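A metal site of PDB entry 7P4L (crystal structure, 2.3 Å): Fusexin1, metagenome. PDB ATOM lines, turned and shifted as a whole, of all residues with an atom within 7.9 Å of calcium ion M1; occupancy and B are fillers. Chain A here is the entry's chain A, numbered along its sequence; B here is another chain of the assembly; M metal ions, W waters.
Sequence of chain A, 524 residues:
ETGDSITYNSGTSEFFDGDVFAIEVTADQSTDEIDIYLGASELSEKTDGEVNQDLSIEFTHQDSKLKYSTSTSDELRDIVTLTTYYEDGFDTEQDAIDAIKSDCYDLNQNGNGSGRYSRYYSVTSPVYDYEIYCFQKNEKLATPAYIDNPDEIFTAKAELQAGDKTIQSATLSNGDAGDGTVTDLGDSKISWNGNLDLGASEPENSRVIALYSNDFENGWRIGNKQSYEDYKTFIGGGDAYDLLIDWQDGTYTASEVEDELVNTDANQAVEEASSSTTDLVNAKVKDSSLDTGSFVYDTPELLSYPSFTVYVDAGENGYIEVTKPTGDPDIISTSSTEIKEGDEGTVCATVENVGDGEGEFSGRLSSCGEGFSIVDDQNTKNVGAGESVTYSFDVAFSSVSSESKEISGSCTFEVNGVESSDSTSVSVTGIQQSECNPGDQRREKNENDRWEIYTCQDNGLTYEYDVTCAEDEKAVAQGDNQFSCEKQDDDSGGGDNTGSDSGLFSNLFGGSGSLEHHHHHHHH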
ATOM      1  N   LEU A 198     -26.136  -5.599  27.608  1.00  0.00           N
ATOM      2  CA  LEU A 198     -25.383  -4.988  26.517  1.00  0.00           C
ATOM      3  C   LEU A 198     -23.942  -5.470  26.431  1.00  0.00           C
ATOM      4  O   LEU A 198     -23.290  -5.244  25.396  1.00  0.00           O
ATOM      5  CB  LEU A 198     -25.372  -3.458  26.653  1.00  0.00           C
ATOM      6  CG  LEU A 198     -26.754  -2.791  26.723  1.00  0.00           C
ATOM      7  CD1 LEU A 198     -26.608  -1.273  26.673  1.00  0.00           C
ATOM      8  CD2 LEU A 198     -27.647  -3.304  25.617  1.00  0.00           C
ATOM      9  N   GLY A 199     -23.438  -6.150  27.447  1.00  0.00           N
ATOM     10  CA  GLY A 199     -22.061  -6.613  27.440  1.00  0.00           C
ATOM     11  C   GLY A 199     -21.062  -5.670  28.070  1.00  0.00           C
ATOM     12  O   GLY A 199     -19.876  -6.003  28.136  1.00  0.00           O
ATOM     13  N   ALA A 200     -21.494  -4.484  28.489  1.00  0.00           N
ATOM     14  CA  ALA A 200     -20.585  -3.546  29.140  1.00  0.00           C
ATOM     15  C   ALA A 200     -20.128  -4.073  30.494  1.00  0.00           C
ATOM     16  O   ALA A 200     -20.835  -4.830  31.174  1.00  0.00           O
ATOM     17  CB  ALA A 200     -21.281  -2.196  29.327  1.00  0.00           C
ATOM     18  N   SER A 201     -18.921  -3.680  30.883  1.00  0.00           N
ATOM     19  CA  SER A 201     -18.314  -4.140  32.124  1.00  0.00           C
ATOM     20  C   SER A 201     -18.654  -3.203  33.293  1.00  0.00           C
ATOM     21  O   SER A 201     -19.086  -2.062  33.096  1.00  0.00           O
ATOM     22  CB  SER A 201     -16.789  -4.235  31.955  1.00  0.00           C
ATOM     23  OG  SER A 201     -16.254  -3.006  31.508  1.00  0.00           O
ATOM     24  N   GLU A 301     -22.263   4.984  30.946  1.00  0.00           N
ATOM     25  CA  GLU A 301     -22.849   4.250  29.836  1.00  0.00           C
ATOM     26  C   GLU A 301     -24.025   3.408  30.333  1.00  0.00           C
ATOM     27  O   GLU A 301     -24.136   3.119  31.527  1.00  0.00           O
ATOM     28  CB  GLU A 301     -21.767   3.352  29.205  1.00  0.00           C
ATOM     29  CG  GLU A 301     -22.152   2.525  28.006  1.00  0.00           C
ATOM     30  CD  GLU A 301     -21.023   1.566  27.610  1.00  0.00           C
ATOM     31  OE1 GLU A 301     -20.040   1.441  28.377  1.00  0.00           O
ATOM     32  OE2 GLU A 301     -21.117   0.949  26.528  1.00  0.00           O
ATOM     33  N   LEU A 302     -24.902   3.035  29.412  1.00  0.00           N
ATOM     34  CA  LEU A 302     -25.980   2.112  29.741  1.00  0.00           C
ATOM     35  C   LEU A 302     -25.437   0.687  29.822  1.00  0.00           C
ATOM     36  O   LEU A 302     -24.650   0.264  28.979  1.00  0.00           O
ATOM     37  CB  LEU A 302     -27.102   2.177  28.708  1.00  0.00           C
ATOM     38  CG  LEU A 302     -27.940   3.456  28.675  1.00  0.00           C
ATOM     39  CD1 LEU A 302     -28.920   3.400  27.502  1.00  0.00           C
ATOM     40  CD2 LEU A 302     -28.692   3.650  29.984  1.00  0.00           C
ATOM     41  N   LEU A 303     -25.898  -0.062  30.832  1.00  0.00           N
ATOM     42  CA  LEU A 303     -25.448  -1.422  31.024  1.00  0.00           C
ATOM     43  C   LEU A 303     -26.449  -2.458  30.534  1.00  0.00           C
ATOM     44  O   LEU A 303     -26.073  -3.608  30.328  1.00  0.00           O
ATOM     45  CB  LEU A 303     -25.164  -1.687  32.508  1.00  0.00           C
ATOM     46  CG  LEU A 303     -24.115  -0.788  33.159  1.00  0.00           C
ATOM     47  CD1 LEU A 303     -24.004  -1.090  34.639  1.00  0.00           C
ATOM     48  CD2 LEU A 303     -22.785  -0.942  32.464  1.00  0.00           C
ATOM     49  N   VAL A 375     -10.819  -2.338  22.965  1.00  0.00           N
ATOM     50  CA  VAL A 375     -11.155  -2.989  24.223  1.00  0.00           C
ATOM     51  C   VAL A 375     -12.432  -2.379  24.770  1.00  0.00           C
ATOM     52  O   VAL A 375     -12.588  -2.208  25.991  1.00  0.00           O
ATOM     53  CB  VAL A 375      -9.995  -2.894  25.238  1.00  0.00           C
ATOM     54  CG1 VAL A 375      -8.800  -3.704  24.743  1.00  0.00           C
ATOM     55  CG2 VAL A 375      -9.586  -1.446  25.471  1.00  0.00           C
ATOM     56  N   ASP A 376     -13.355  -2.039  23.872  1.00  0.00           N
ATOM     57  CA  ASP A 376     -14.623  -1.421  24.229  1.00  0.00           C
ATOM     58  C   ASP A 376     -15.717  -1.986  23.329  1.00  0.00           C
ATOM     59  O   ASP A 376     -15.443  -2.570  22.280  1.00  0.00           O
ATOM     60  CB  ASP A 376     -14.551   0.105  24.096  1.00  0.00           C
ATOM     61  CG  ASP A 376     -15.357   0.835  25.160  1.00  0.00           C
ATOM     62  OD1 ASP A 376     -16.262   0.225  25.774  1.00  0.00           O
ATOM     63  OD2 ASP A 376     -15.075   2.037  25.387  1.00  0.00           O
ATOM     64  N   ASP A 377     -16.961  -1.804  23.752  1.00  0.00           N
ATOM     65  CA  ASP A 377     -18.130  -2.152  22.967  1.00  0.00           C
ATOM     66  C   ASP A 377     -18.692  -0.909  22.288  1.00  0.00           C
ATOM     67  O   ASP A 377     -18.209   0.208  22.462  1.00  0.00           O
ATOM     68  CB  ASP A 377     -19.190  -2.813  23.845  1.00  0.00           C
ATOM     69  CG  ASP A 377     -19.612  -1.938  25.008  1.00  0.00           C
ATOM     70  OD1 ASP A 377     -18.754  -1.246  25.583  1.00  0.00           O
ATOM     71  OD2 ASP A 377     -20.817  -1.926  25.343  1.00  0.00           O
ATOM     72  N   GLN A 378     -19.727  -1.112  21.481  1.00  0.00           N
ATOM     73  CA  GLN A 378     -20.409   0.009  20.848  1.00  0.00           C
ATOM     74  C   GLN A 378     -21.195   0.793  21.893  1.00  0.00           C
ATOM     75  O   GLN A 378     -21.452   0.318  23.001  1.00  0.00           O
ATOM     76  CB  GLN A 378     -21.356  -0.486  19.747  1.00  0.00           C
ATOM     77  CG  GLN A 378     -22.509  -1.357  20.224  1.00  0.00           C
ATOM     78  CD  GLN A 378     -23.687  -0.567  20.771  1.00  0.00           C
ATOM     79  OE1 GLN A 378     -24.235   0.300  20.100  1.00  0.00           O
ATOM     80  NE2 GLN A 378     -24.068  -0.853  22.006  1.00  0.00           N
ATOM     81  N   ASN A 379     -21.590   2.009  21.512  1.00  0.00           N
ATOM     82  CA  ASN A 379     -22.490   2.820  22.324  1.00  0.00           C
ATOM     83  C   ASN A 379     -23.547   3.435  21.410  1.00  0.00           C
ATOM     84  O   ASN A 379     -23.206   3.995  20.362  1.00  0.00           O
ATOM     85  CB  ASN A 379     -21.717   3.911  23.073  1.00  0.00           C
ATOM     86  CG  ASN A 379     -22.403   4.330  24.357  1.00  0.00           C
ATOM     87  OD1 ASN A 379     -23.076   3.535  25.001  1.00  0.00           O
ATOM     88  ND2 ASN A 379     -22.225   5.589  24.736  1.00  0.00           N
ATOM     89  N   SER A 392     -16.941   7.984  22.849  1.00  0.00           N
ATOM     90  CA  SER A 392     -15.613   7.732  23.417  1.00  0.00           C
ATOM     91  C   SER A 392     -15.429   6.228  23.580  1.00  0.00           C
ATOM     92  O   SER A 392     -16.296   5.546  24.127  1.00  0.00           O
ATOM     93  CB  SER A 392     -15.464   8.432  24.773  1.00  0.00           C
ATOM     94  OG  SER A 392     -14.178   8.222  25.327  1.00  0.00           O
ATOM     95  N   PHE A 393     -14.307   5.712  23.084  1.00  0.00           N
ATOM     96  CA  PHE A 393     -14.060   4.272  23.075  1.00  0.00           C
ATOM     97  C   PHE A 393     -12.648   3.963  23.545  1.00  0.00           C
ATOM     98  O   PHE A 393     -11.701   4.690  23.217  1.00  0.00           O
ATOM     99  CB  PHE A 393     -14.305   3.681  21.679  1.00  0.00           C
ATOM    100  CG  PHE A 393     -15.698   3.893  21.186  1.00  0.00           C
ATOM    101  CD1 PHE A 393     -16.741   3.145  21.691  1.00  0.00           C
ATOM    102  CD2 PHE A 393     -15.976   4.862  20.232  1.00  0.00           C
ATOM    103  CE1 PHE A 393     -18.024   3.346  21.255  1.00  0.00           C
ATOM    104  CE2 PHE A 393     -17.253   5.072  19.794  1.00  0.00           C
ATOM    105  CZ  PHE A 393     -18.282   4.306  20.307  1.00  0.00           C
ATOM    106  N   ASP A 394     -12.512   2.889  24.327  1.00  0.00           N
ATOM    107  CA  ASP A 394     -11.228   2.511  24.900  1.00  0.00           C
ATOM    108  C   ASP A 394     -10.398   1.713  23.893  1.00  0.00           C
ATOM    109  O   ASP A 394     -10.860   0.694  23.360  1.00  0.00           O
ATOM    110  CB  ASP A 394     -11.424   1.685  26.171  1.00  0.00           C
ATOM    111  CG  ASP A 394     -12.009   2.501  27.311  1.00  0.00           C
ATOM    112  OD1 ASP A 394     -11.904   3.748  27.290  1.00  0.00           O
ATOM    113  OD2 ASP A 394     -12.582   1.898  28.249  1.00  0.00           O
ATOM    114  N   ASP B 151     -15.330  -6.576  28.673  1.00  0.00           N
ATOM    115  CA  ASP B 151     -16.567  -6.403  27.930  1.00  0.00           C
ATOM    116  C   ASP B 151     -16.891  -7.693  27.195  1.00  0.00           C
ATOM    117  O   ASP B 151     -15.996  -8.389  26.705  1.00  0.00           O
ATOM    118  CB  ASP B 151     -16.467  -5.253  26.926  1.00  0.00           C
ATOM    119  CG  ASP B 151     -16.150  -3.921  27.575  1.00  0.00           C
ATOM    120  OD1 ASP B 151     -16.963  -3.441  28.406  1.00  0.00           O
ATOM    121  OD2 ASP B 151     -15.092  -3.331  27.260  1.00  0.00           O
HETATM  122 CA    CA M   1     -18.221   0.577  26.917  1.00  0.00          CA
HETATM  123 CA    CA M   2     -13.392  -2.104  28.344  1.00  0.00          CA
HETATM  124  O   HOH W   1     -17.117  -0.860  28.601  1.00  0.00           O
HETATM  125  O   HOH W   2     -16.533   2.858  26.935  1.00  0.00           O
HETATM  126  O   HOH W   3     -18.664   1.362  24.606  1.00  0.00           O
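OD1 of Asp 376 is bound to calcium ion M1, 2.3 Å away.
Calcium ion M1 is bound by OD1 of Asp 377, 2.3 Å away.
Calcium ion M1 is bound by water W1, 2.5 Å away.
Water W3 binds calcium ion M1 (2.5 Å).
The side-chain carboxylate (OE1) of Glu 301 binds calcium ion M1 (2.5 Å).
Water W2 binds calcium ion M1 (2.8 Å).
Slightly farther from calcium ion M1 lies the side-chain carboxylate (OE2) of Glu 301 (2.9 Å).
Of the 16 residues printed, 3 come within 4 Å of calcium ion M1.
The nearest printed residue that does not touch calcium ion M1 is Asp 151 of chain B (4.5 Å).
OD2 of Asp 376 lies within hydrogen-bond range of N of Asp 394 (2.9 Å).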
